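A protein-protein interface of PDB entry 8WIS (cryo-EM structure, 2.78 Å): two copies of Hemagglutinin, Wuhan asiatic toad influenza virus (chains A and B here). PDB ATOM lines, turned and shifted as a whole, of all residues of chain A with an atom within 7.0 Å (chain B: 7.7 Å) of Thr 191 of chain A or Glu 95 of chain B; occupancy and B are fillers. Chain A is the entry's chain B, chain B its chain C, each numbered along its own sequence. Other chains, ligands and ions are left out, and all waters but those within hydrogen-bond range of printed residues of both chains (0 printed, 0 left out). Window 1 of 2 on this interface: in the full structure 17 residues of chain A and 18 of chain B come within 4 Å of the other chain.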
ATOM      1  N   GLU A 152     -18.494   3.915   1.614  1.00  0.00           N
ATOM      2  CA  GLU A 152     -19.168   2.624   1.574  1.00  0.00           C
ATOM      3  C   GLU A 152     -18.458   1.733   0.566  1.00  0.00           C
ATOM      4  O   GLU A 152     -18.128   2.187  -0.534  1.00  0.00           O
ATOM      5  CB  GLU A 152     -20.632   2.785   1.159  1.00  0.00           C
ATOM      6  CG  GLU A 152     -21.530   3.516   2.138  1.00  0.00           C
ATOM      7  CD  GLU A 152     -21.932   2.659   3.315  1.00  0.00           C
ATOM      8  OE1 GLU A 152     -22.018   1.425   3.149  1.00  0.00           O
ATOM      9  OE2 GLU A 152     -22.194   3.223   4.398  1.00  0.00           O
ATOM     10  N   TYR A 163      -7.214   1.801  10.011  1.00  0.00           N
ATOM     11  CA  TYR A 163      -7.655   3.163   9.753  1.00  0.00           C
ATOM     12  C   TYR A 163      -7.269   4.041  10.931  1.00  0.00           C
ATOM     13  O   TYR A 163      -6.992   3.554  12.025  1.00  0.00           O
ATOM     14  CB  TYR A 163      -9.170   3.231   9.538  1.00  0.00           C
ATOM     15  CG  TYR A 163      -9.954   2.952  10.798  1.00  0.00           C
ATOM     16  CD1 TYR A 163     -10.199   1.654  11.210  1.00  0.00           C
ATOM     17  CD2 TYR A 163     -10.442   3.989  11.579  1.00  0.00           C
ATOM     18  CE1 TYR A 163     -10.907   1.395  12.361  1.00  0.00           C
ATOM     19  CE2 TYR A 163     -11.149   3.737  12.731  1.00  0.00           C
ATOM     20  CZ  TYR A 163     -11.379   2.440  13.116  1.00  0.00           C
ATOM     21  OH  TYR A 163     -12.087   2.183  14.265  1.00  0.00           O
ATOM     22  N   ARG A 189     -14.973   6.427  12.783  1.00  0.00           N
ATOM     23  CA  ARG A 189     -15.730   5.230  13.106  1.00  0.00           C
ATOM     24  C   ARG A 189     -15.694   4.239  11.951  1.00  0.00           C
ATOM     25  O   ARG A 189     -15.703   4.622  10.779  1.00  0.00           O
ATOM     26  CB  ARG A 189     -17.181   5.571  13.443  1.00  0.00           C
ATOM     27  CG  ARG A 189     -17.330   6.723  14.415  1.00  0.00           C
ATOM     28  CD  ARG A 189     -18.491   6.498  15.361  1.00  0.00           C
ATOM     29  NE  ARG A 189     -18.571   7.539  16.376  1.00  0.00           N
ATOM     30  CZ  ARG A 189     -19.430   7.534  17.386  1.00  0.00           C
ATOM     31  NH1 ARG A 189     -20.305   6.555  17.543  1.00  0.00           N
ATOM     32  NH2 ARG A 189     -19.409   8.536  18.260  1.00  0.00           N
ATOM     33  N   PHE A 190     -15.664   2.958  12.305  1.00  0.00           N
ATOM     34  CA  PHE A 190     -15.632   1.859  11.354  1.00  0.00           C
ATOM     35  C   PHE A 190     -16.771   0.910  11.685  1.00  0.00           C
ATOM     36  O   PHE A 190     -16.933   0.513  12.844  1.00  0.00           O
ATOM     37  CB  PHE A 190     -14.288   1.128  11.411  1.00  0.00           C
ATOM     38  CG  PHE A 190     -14.115   0.084  10.349  1.00  0.00           C
ATOM     39  CD1 PHE A 190     -14.579  -1.204  10.540  1.00  0.00           C
ATOM     40  CD2 PHE A 190     -13.477   0.390   9.162  1.00  0.00           C
ATOM     41  CE1 PHE A 190     -14.417  -2.162   9.565  1.00  0.00           C
ATOM     42  CE2 PHE A 190     -13.312  -0.565   8.185  1.00  0.00           C
ATOM     43  CZ  PHE A 190     -13.783  -1.841   8.385  1.00  0.00           C
ATOM     44  N   THR A 191     -17.553   0.546  10.671  1.00  0.00           N
ATOM     45  CA  THR A 191     -18.720  -0.321  10.837  1.00  0.00           C
ATOM     46  C   THR A 191     -18.675  -1.396   9.755  1.00  0.00           C
ATOM     47  O   THR A 191     -19.141  -1.182   8.633  1.00  0.00           O
ATOM     48  CB  THR A 191     -20.011   0.482  10.775  1.00  0.00           C
ATOM     49  OG1 THR A 191     -19.981   1.512  11.770  1.00  0.00           O
ATOM     50  CG2 THR A 191     -21.206  -0.420  11.026  1.00  0.00           C
ATOM     51  N   GLY A 192     -18.106  -2.547  10.096  1.00  0.00           N
ATOM     52  CA  GLY A 192     -18.104  -3.691   9.206  1.00  0.00           C
ATOM     53  C   GLY A 192     -18.784  -4.879   9.848  1.00  0.00           C
ATOM     54  O   GLY A 192     -19.978  -4.826  10.156  1.00  0.00           O
ATOM     55  N   SER A 193     -18.034  -5.963  10.054  1.00  0.00           N
ATOM     56  CA  SER A 193     -18.550  -7.078  10.838  1.00  0.00           C
ATOM     57  C   SER A 193     -18.735  -6.706  12.302  1.00  0.00           C
ATOM     58  O   SER A 193     -19.432  -7.421  13.029  1.00  0.00           O
ATOM     59  CB  SER A 193     -17.617  -8.281  10.720  1.00  0.00           C
ATOM     60  OG  SER A 193     -18.067  -9.352  11.529  1.00  0.00           O
ATOM     61  N   SER A 194     -18.123  -5.610  12.744  1.00  0.00           N
ATOM     62  CA  SER A 194     -18.265  -5.120  14.106  1.00  0.00           C
ATOM     63  C   SER A 194     -18.113  -3.607  14.085  1.00  0.00           C
ATOM     64  O   SER A 194     -17.902  -3.002  13.032  1.00  0.00           O
ATOM     65  CB  SER A 194     -17.237  -5.754  15.048  1.00  0.00           C
ATOM     66  OG  SER A 194     -17.217  -7.162  14.908  1.00  0.00           O
ATOM     67  N   GLU A 195     -18.230  -2.999  15.261  1.00  0.00           N
ATOM     68  CA  GLU A 195     -18.142  -1.553  15.401  1.00  0.00           C
ATOM     69  C   GLU A 195     -16.843  -1.179  16.103  1.00  0.00           C
ATOM     70  O   GLU A 195     -16.461  -1.815  17.089  1.00  0.00           O
ATOM     71  CB  GLU A 195     -19.341  -1.011  16.181  1.00  0.00           C
ATOM     72  CG  GLU A 195     -19.312   0.493  16.405  1.00  0.00           C
ATOM     73  CD  GLU A 195     -19.475   1.286  15.121  1.00  0.00           C
ATOM     74  OE1 GLU A 195     -19.172   2.498  15.129  1.00  0.00           O
ATOM     75  OE2 GLU A 195     -19.920   0.706  14.108  1.00  0.00           O
ATOM     76  N   SER A 196     -16.170  -0.150  15.590  1.00  0.00           N
ATOM     77  CA  SER A 196     -14.960   0.365  16.213  1.00  0.00           C
ATOM     78  C   SER A 196     -14.909   1.873  16.023  1.00  0.00           C
ATOM     79  O   SER A 196     -15.540   2.424  15.120  1.00  0.00           O
ATOM     80  CB  SER A 196     -13.701  -0.288  15.633  1.00  0.00           C
ATOM     81  OG  SER A 196     -13.703  -1.684  15.867  1.00  0.00           O
ATOM     82  N   ARG A 233     -12.836  -5.084  11.320  1.00  0.00           N
ATOM     83  CA  ARG A 233     -13.054  -6.369  10.671  1.00  0.00           C
ATOM     84  C   ARG A 233     -14.211  -6.279   9.687  1.00  0.00           C
ATOM     85  O   ARG A 233     -15.201  -5.587   9.939  1.00  0.00           O
ATOM     86  CB  ARG A 233     -13.333  -7.460  11.705  1.00  0.00           C
ATOM     87  CG  ARG A 233     -12.228  -7.625  12.727  1.00  0.00           C
ATOM     88  CD  ARG A 233     -11.198  -8.637  12.267  1.00  0.00           C
ATOM     89  NE  ARG A 233     -11.785  -9.951  12.041  1.00  0.00           N
ATOM     90  CZ  ARG A 233     -11.374 -10.805  11.115  1.00  0.00           C
ATOM     91  NH1 ARG A 233     -10.368 -10.517  10.306  1.00  0.00           N
ATOM     92  NH2 ARG A 233     -11.987 -11.979  10.997  1.00  0.00           N
ATOM     93  N   VAL A 234     -14.077  -6.981   8.562  1.00  0.00           N
ATOM     94  CA  VAL A 234     -15.097  -6.980   7.519  1.00  0.00           C
ATOM     95  C   VAL A 234     -15.511  -8.409   7.198  1.00  0.00           C
ATOM     96  O   VAL A 234     -14.903  -9.369   7.682  1.00  0.00           O
ATOM     97  CB  VAL A 234     -14.599  -6.262   6.253  1.00  0.00           C
ATOM     98  CG1 VAL A 234     -14.104  -4.872   6.589  1.00  0.00           C
ATOM     99  CG2 VAL A 234     -13.505  -7.071   5.589  1.00  0.00           C
ATOM    100  N   THR A 239     -21.104  -5.199   3.431  1.00  0.00           N
ATOM    101  CA  THR A 239     -20.549  -3.904   3.060  1.00  0.00           C
ATOM    102  C   THR A 239     -20.046  -3.187   4.305  1.00  0.00           C
ATOM    103  O   THR A 239     -20.739  -3.146   5.325  1.00  0.00           O
ATOM    104  CB  THR A 239     -21.605  -3.054   2.351  1.00  0.00           C
ATOM    105  OG1 THR A 239     -21.932  -3.648   1.090  1.00  0.00           O
ATOM    106  CG2 THR A 239     -21.098  -1.642   2.121  1.00  0.00           C
ATOM    107  N   PHE A 240     -18.846  -2.621   4.217  1.00  0.00           N
ATOM    108  CA  PHE A 240     -18.246  -1.884   5.316  1.00  0.00           C
ATOM    109  C   PHE A 240     -18.191  -0.397   4.989  1.00  0.00           C
ATOM    110  O   PHE A 240     -18.045   0.000   3.828  1.00  0.00           O
ATOM    111  CB  PHE A 240     -16.839  -2.407   5.633  1.00  0.00           C
ATOM    112  CG  PHE A 240     -15.792  -1.986   4.643  1.00  0.00           C
ATOM    113  CD1 PHE A 240     -15.589  -2.710   3.483  1.00  0.00           C
ATOM    114  CD2 PHE A 240     -14.995  -0.882   4.882  1.00  0.00           C
ATOM    115  CE1 PHE A 240     -14.624  -2.330   2.574  1.00  0.00           C
ATOM    116  CE2 PHE A 240     -14.030  -0.497   3.975  1.00  0.00           C
ATOM    117  CZ  PHE A 240     -13.844  -1.223   2.822  1.00  0.00           C
ATOM    118  N   SER A 241     -18.306   0.420   6.033  1.00  0.00           N
ATOM    119  CA  SER A 241     -18.349   1.868   5.901  1.00  0.00           C
ATOM    120  C   SER A 241     -17.388   2.511   6.888  1.00  0.00           C
ATOM    121  O   SER A 241     -17.262   2.061   8.029  1.00  0.00           O
ATOM    122  CB  SER A 241     -19.759   2.401   6.140  1.00  0.00           C
ATOM    123  OG  SER A 241     -19.981   2.642   7.516  1.00  0.00           O
ATOM    124  N   ILE A 242     -16.719   3.569   6.439  1.00  0.00           N
ATOM    125  CA  ILE A 242     -15.786   4.332   7.263  1.00  0.00           C
ATOM    126  C   ILE A 242     -16.197   5.795   7.231  1.00  0.00           C
ATOM    127  O   ILE A 242     -16.425   6.356   6.155  1.00  0.00           O
ATOM    128  CB  ILE A 242     -14.333   4.172   6.782  1.00  0.00           C
ATOM    129  CG1 ILE A 242     -14.015   2.707   6.493  1.00  0.00           C
ATOM    130  CG2 ILE A 242     -13.371   4.726   7.815  1.00  0.00           C
ATOM    131  CD1 ILE A 242     -12.583   2.467   6.086  1.00  0.00           C
ATOM    132  N   SER A 243     -16.281   6.416   8.404  1.00  0.00           N
ATOM    133  CA  SER A 243     -16.616   7.833   8.508  1.00  0.00           C
ATOM    134  C   SER A 243     -15.327   8.642   8.427  1.00  0.00           C
ATOM    135  O   SER A 243     -14.526   8.639   9.366  1.00  0.00           O
ATOM    136  CB  SER A 243     -17.362   8.117   9.805  1.00  0.00           C
ATOM    137  OG  SER A 243     -17.549   9.508   9.985  1.00  0.00           O
ATOM    138  N   MET B  82     -35.891  -2.789   7.879  1.00  0.00           N
ATOM    139  CA  MET B  82     -35.513  -1.811   8.893  1.00  0.00           C
ATOM    140  C   MET B  82     -35.406  -0.404   8.322  1.00  0.00           C
ATOM    141  O   MET B  82     -35.808   0.561   8.981  1.00  0.00           O
ATOM    142  CB  MET B  82     -34.190  -2.214   9.541  1.00  0.00           C
ATOM    143  CG  MET B  82     -33.737  -1.285  10.651  1.00  0.00           C
ATOM    144  SD  MET B  82     -34.349  -1.793  12.266  1.00  0.00           S
ATOM    145  CE  MET B  82     -33.631  -3.426  12.389  1.00  0.00           C
ATOM    146  N   TYR B  92     -31.991   7.643  13.250  1.00  0.00           N
ATOM    147  CA  TYR B  92     -30.710   6.954  13.250  1.00  0.00           C
ATOM    148  C   TYR B  92     -30.685   5.971  14.410  1.00  0.00           C
ATOM    149  O   TYR B  92     -31.153   6.288  15.509  1.00  0.00           O
ATOM    150  CB  TYR B  92     -29.543   7.933  13.376  1.00  0.00           C
ATOM    151  CG  TYR B  92     -28.196   7.259  13.488  1.00  0.00           C
ATOM    152  CD1 TYR B  92     -27.601   6.668  12.384  1.00  0.00           C
ATOM    153  CD2 TYR B  92     -27.527   7.202  14.700  1.00  0.00           C
ATOM    154  CE1 TYR B  92     -26.372   6.048  12.484  1.00  0.00           C
ATOM    155  CE2 TYR B  92     -26.301   6.583  14.810  1.00  0.00           C
ATOM    156  CZ  TYR B  92     -25.727   6.009  13.699  1.00  0.00           C
ATOM    157  OH  TYR B  92     -24.504   5.392  13.806  1.00  0.00           O
ATOM    158  N   LEU B  93     -30.144   4.780  14.166  1.00  0.00           N
ATOM    159  CA  LEU B  93     -30.128   3.716  15.159  1.00  0.00           C
ATOM    160  C   LEU B  93     -28.741   3.104  15.262  1.00  0.00           C
ATOM    161  O   LEU B  93     -28.096   2.825  14.248  1.00  0.00           O
ATOM    162  CB  LEU B  93     -31.140   2.619  14.818  1.00  0.00           C
ATOM    163  CG  LEU B  93     -32.543   3.063  14.417  1.00  0.00           C
ATOM    164  CD1 LEU B  93     -33.270   1.930  13.721  1.00  0.00           C
ATOM    165  CD2 LEU B  93     -33.316   3.534  15.630  1.00  0.00           C
ATOM    166  N   THR B  94     -28.295   2.890  16.495  1.00  0.00           N
ATOM    167  CA  THR B  94     -27.049   2.190  16.749  1.00  0.00           C
ATOM    168  C   THR B  94     -27.205   0.714  16.382  1.00  0.00           C
ATOM    169  O   THR B  94     -28.318   0.190  16.283  1.00  0.00           O
ATOM    170  CB  THR B  94     -26.655   2.358  18.220  1.00  0.00           C
ATOM    171  OG1 THR B  94     -26.634   3.752  18.540  1.00  0.00           O
ATOM    172  CG2 THR B  94     -25.274   1.789  18.501  1.00  0.00           C
ATOM    173  N   GLU B  95     -26.070   0.045  16.149  1.00  0.00           N
ATOM    174  CA  GLU B  95     -26.099  -1.371  15.790  1.00  0.00           C
ATOM    175  C   GLU B  95     -26.856  -2.194  16.823  1.00  0.00           C
ATOM    176  O   GLU B  95     -27.620  -3.100  16.468  1.00  0.00           O
ATOM    177  CB  GLU B  95     -24.674  -1.895  15.630  1.00  0.00           C
ATOM    178  CG  GLU B  95     -23.819  -1.096  14.662  1.00  0.00           C
ATOM    179  CD  GLU B  95     -24.363  -1.116  13.248  1.00  0.00           C
ATOM    180  OE1 GLU B  95     -24.541  -2.219  12.693  1.00  0.00           O
ATOM    181  OE2 GLU B  95     -24.611  -0.026  12.690  1.00  0.00           O
ATOM    182  N   LYS B  96     -26.660  -1.895  18.110  1.00  0.00           N
ATOM    183  CA  LYS B  96     -27.433  -2.565  19.150  1.00  0.00           C
ATOM    184  C   LYS B  96     -28.920  -2.280  18.995  1.00  0.00           C
ATOM    185  O   LYS B  96     -29.757  -3.176  19.163  1.00  0.00           O
ATOM    186  CB  LYS B  96     -26.947  -2.122  20.528  1.00  0.00           C
ATOM    187  CG  LYS B  96     -25.837  -2.976  21.100  1.00  0.00           C
ATOM    188  CD  LYS B  96     -25.275  -2.360  22.365  1.00  0.00           C
ATOM    189  CE  LYS B  96     -26.375  -2.030  23.355  1.00  0.00           C
ATOM    190  NZ  LYS B  96     -25.849  -1.268  24.518  1.00  0.00           N
ATOM    191  N   ALA B  97     -29.266  -1.031  18.676  1.00  0.00           N
ATOM    192  CA  ALA B  97     -30.666  -0.684  18.476  1.00  0.00           C
ATOM    193  C   ALA B  97     -31.269  -1.487  17.336  1.00  0.00           C
ATOM    194  O   ALA B  97     -32.403  -1.958  17.438  1.00  0.00           O
ATOM    195  CB  ALA B  97     -30.806   0.813  18.214  1.00  0.00           C
ATOM    196  N   LYS B  98     -30.526  -1.658  16.240  1.00  0.00           N
ATOM    197  CA  LYS B  98     -31.023  -2.464  15.128  1.00  0.00           C
ATOM    198  C   LYS B  98     -31.198  -3.920  15.542  1.00  0.00           C
ATOM    199  O   LYS B  98     -32.232  -4.542  15.260  1.00  0.00           O
ATOM    200  CB  LYS B  98     -30.067  -2.359  13.942  1.00  0.00           C
ATOM    201  CG  LYS B  98     -30.100  -1.026  13.225  1.00  0.00           C
ATOM    202  CD  LYS B  98     -29.322  -1.092  11.925  1.00  0.00           C
ATOM    203  CE  LYS B  98     -28.697   0.247  11.593  1.00  0.00           C
ATOM    204  NZ  LYS B  98     -27.538   0.099  10.676  1.00  0.00           N
ATOM    205  N   SER B  99     -30.191  -4.477  16.219  1.00  0.00           N
ATOM    206  CA  SER B  99     -30.242  -5.882  16.605  1.00  0.00           C
ATOM    207  C   SER B  99     -31.386  -6.161  17.568  1.00  0.00           C
ATOM    208  O   SER B  99     -31.917  -7.276  17.590  1.00  0.00           O
ATOM    209  CB  SER B  99     -28.915  -6.306  17.230  1.00  0.00           C
ATOM    210  OG  SER B  99     -27.884  -6.340  16.260  1.00  0.00           O
ATOM    211  N   TRP B 100     -31.777  -5.174  18.371  1.00  0.00           N
ATOM    212  CA  TRP B 100     -32.869  -5.390  19.310  1.00  0.00           C
ATOM    213  C   TRP B 100     -34.228  -5.003  18.745  1.00  0.00           C
ATOM    214  O   TRP B 100     -35.246  -5.557  19.177  1.00  0.00           O
ATOM    215  CB  TRP B 100     -32.606  -4.624  20.606  1.00  0.00           C
ATOM    216  CG  TRP B 100     -31.692  -5.360  21.526  1.00  0.00           C
ATOM    217  CD1 TRP B 100     -30.394  -5.056  21.805  1.00  0.00           C
ATOM    218  CD2 TRP B 100     -31.998  -6.540  22.275  1.00  0.00           C
ATOM    219  NE1 TRP B 100     -29.876  -5.967  22.690  1.00  0.00           N
ATOM    220  CE2 TRP B 100     -30.841  -6.890  22.993  1.00  0.00           C
ATOM    221  CE3 TRP B 100     -33.141  -7.330  22.411  1.00  0.00           C
ATOM    222  CZ2 TRP B 100     -30.793  -7.996  23.834  1.00  0.00           C
ATOM    223  CZ3 TRP B 100     -33.091  -8.427  23.246  1.00  0.00           C
ATOM    224  CH2 TRP B 100     -31.926  -8.750  23.947  1.00  0.00           C
ATOM    225  N   MET B 101     -34.273  -4.065  17.799  1.00  0.00           N
ATOM    226  CA  MET B 101     -35.515  -3.726  17.120  1.00  0.00           C
ATOM    227  C   MET B 101     -35.924  -4.792  16.122  1.00  0.00           C
ATOM    228  O   MET B 101     -37.102  -4.867  15.761  1.00  0.00           O
ATOM    229  CB  MET B 101     -35.377  -2.381  16.405  1.00  0.00           C
ATOM    230  CG  MET B 101     -35.542  -1.172  17.303  1.00  0.00           C
ATOM    231  SD  MET B 101     -35.462   0.374  16.385  1.00  0.00           S
ATOM    232  CE  MET B 101     -36.498   1.429  17.391  1.00  0.00           C
ATOM    233  N   GLU B 210     -21.861  12.766  11.146  1.00  0.00           N
ATOM    234  CA  GLU B 210     -22.143  11.456  10.578  1.00  0.00           C
ATOM    235  C   GLU B 210     -23.558  10.991  10.887  1.00  0.00           C
ATOM    236  O   GLU B 210     -24.092  10.154  10.154  1.00  0.00           O
ATOM    237  CB  GLU B 210     -21.136  10.423  11.085  1.00  0.00           C
ATOM    238  CG  GLU B 210     -21.564   9.698  12.345  1.00  0.00           C
ATOM    239  CD  GLU B 210     -20.537   8.695  12.817  1.00  0.00           C
ATOM    240  OE1 GLU B 210     -19.403   8.714  12.295  1.00  0.00           O
ATOM    241  OE2 GLU B 210     -20.865   7.882  13.705  1.00  0.00           O
ATOM    242  N   LYS B 214     -25.739   9.417   7.890  1.00  0.00           N
ATOM    243  CA  LYS B 214     -26.241   8.053   7.992  1.00  0.00           C
ATOM    244  C   LYS B 214     -27.724   7.982   8.331  1.00  0.00           C
ATOM    245  O   LYS B 214     -28.263   6.876   8.429  1.00  0.00           O
ATOM    246  CB  LYS B 214     -25.445   7.277   9.042  1.00  0.00           C
ATOM    247  CG  LYS B 214     -24.010   6.991   8.650  1.00  0.00           C
ATOM    248  CD  LYS B 214     -23.404   5.932   9.551  1.00  0.00           C
ATOM    249  CE  LYS B 214     -21.900   6.088   9.654  1.00  0.00           C
ATOM    250  NZ  LYS B 214     -21.316   5.156  10.655  1.00  0.00           N
ATOM    251  N   LEU B 229     -31.307   7.075  18.319  1.00  0.00           N
ATOM    252  CA  LEU B 229     -31.778   6.142  19.330  1.00  0.00           C
ATOM    253  C   LEU B 229     -30.723   5.092  19.642  1.00  0.00           C
ATOM    254  O   LEU B 229     -29.891   4.744  18.802  1.00  0.00           O
ATOM    255  CB  LEU B 229     -33.070   5.445  18.893  1.00  0.00           C
ATOM    256  CG  LEU B 229     -34.337   6.299  18.869  1.00  0.00           C
ATOM    257  CD1 LEU B 229     -35.540   5.439  18.544  1.00  0.00           C
ATOM    258  CD2 LEU B 229     -34.533   7.020  20.188  1.00  0.00           C
ATOM    259  N   ASP B 230     -30.783   4.595  20.874  1.00  0.00           N
ATOM    260  CA  ASP B 230     -29.928   3.526  21.364  1.00  0.00           C
ATOM    261  C   ASP B 230     -30.748   2.697  22.340  1.00  0.00           C
ATOM    262  O   ASP B 230     -31.790   3.140  22.830  1.00  0.00           O
ATOM    263  CB  ASP B 230     -28.663   4.075  22.031  1.00  0.00           C
ATOM    264  CG  ASP B 230     -27.578   3.031  22.169  1.00  0.00           C
ATOM    265  OD1 ASP B 230     -27.561   2.082  21.361  1.00  0.00           O
ATOM    266  OD2 ASP B 230     -26.737   3.160  23.081  1.00  0.00           O
ATOM    267  N   SER B 231     -30.277   1.487  22.615  1.00  0.00           N
ATOM    268  CA  SER B 231     -31.037   0.515  23.388  1.00  0.00           C
ATOM    269  C   SER B 231     -30.379   0.253  24.735  1.00  0.00           C
ATOM    270  O   SER B 231     -29.153   0.301  24.859  1.00  0.00           O
ATOM    271  CB  SER B 231     -31.173  -0.801  22.622  1.00  0.00           C
ATOM    272  OG  SER B 231     -29.973  -1.547  22.687  1.00  0.00           O
ATOM    273  N   LYS B 407     -25.774 -10.917  15.908  1.00  0.00           N
ATOM    274  CA  LYS B 407     -25.668 -11.337  14.520  1.00  0.00           C
ATOM    275  C   LYS B 407     -25.109 -12.744  14.372  1.00  0.00           C
ATOM    276  O   LYS B 407     -24.953 -13.218  13.242  1.00  0.00           O
ATOM    277  CB  LYS B 407     -24.796 -10.355  13.734  1.00  0.00           C
ATOM    278  CG  LYS B 407     -25.272  -8.915  13.796  1.00  0.00           C
ATOM    279  CD  LYS B 407     -24.885  -8.158  12.538  1.00  0.00           C
ATOM    280  CE  LYS B 407     -23.420  -7.763  12.563  1.00  0.00           C
ATOM    281  NZ  LYS B 407     -23.071  -6.860  11.433  1.00  0.00           N
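No position is printed for both chains. Of the 4 pairs that touch across the chains among the printed residues, none has its exchanged pair printed and touching as well.
The backbone NH (N) of Ser 243 of chain A lies within hydrogen-bond range of the backbone carbonyl oxygen (O) of Arg 189 of chain A (3.0 Å). The side-chain carboxylate (OE2) of Glu 195 of chain A lies within hydrogen-bond range of the side-chain hydroxyl (OG1) of Thr 191 of chain A (2.5 Å). The backbone NH (N) of Thr 191 of chain A lies within hydrogen-bond range of the backbone carbonyl oxygen (O) of Ser 241 of chain A, at 3.1 Å. OE2 of Glu 95 of chain B lies within salt-bridge range of NZ of Lys 98 of chain B (3.6 Å). O of Glu 95 of chain B lies within hydrogen-bond range of OG of Ser 99 of chain B (3.3 Å).
Thr 191 of chain A touches just one residue of chain B: Glu 95. Of the printed residues of chain A, Lys 407 of chain B touches Gly 192. Of the printed residues of chain B, Gly 192 of chain A touches Lys 407. Of the printed residues of chain B, Ser 243 of chain A touches Glu 210. Phe 240 of chain A touches none of the printed residues of chain B. Phe 190 of chain A touches none of the printed residues of chain B. The nearest residue of chain B that does not touch Thr 191 of chain A is Lys 214 of chain B (4.04 Å). The nearest residue of chain A that does not touch Glu 95 of chain B is Glu 195 of chain A (4.3 Å).
Of the 17 printed residues of chain A, 4 touch a printed residue of chain B. Of the 17 printed residues of chain B, 3 touch a printed residue of chain A. Printed residues of chain B that touch a printed residue of chain A: Glu 95, Glu 210 and Lys 407. Among the printed residues, Asp or Glu carboxylates within 4 Å of a Lys or Arg side-chain nitrogen of the other chain: Arg 189 of chain A with Glu 210 of chain B (3.5 Å).
Thr 191 of chain A touches Glu 95 of chain B. Gly 192 of chain A touches Lys 407 of chain B.
The guanidinium group of Arg 189 of chain A lies within salt-bridge range of the side-chain carboxylate of Glu 210 of chain B, 3.5 Å away. OG of Ser 243 of chain A sits at hydrogen-bond distance from OE1 of Glu 210 of chain B (3.1 Å).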
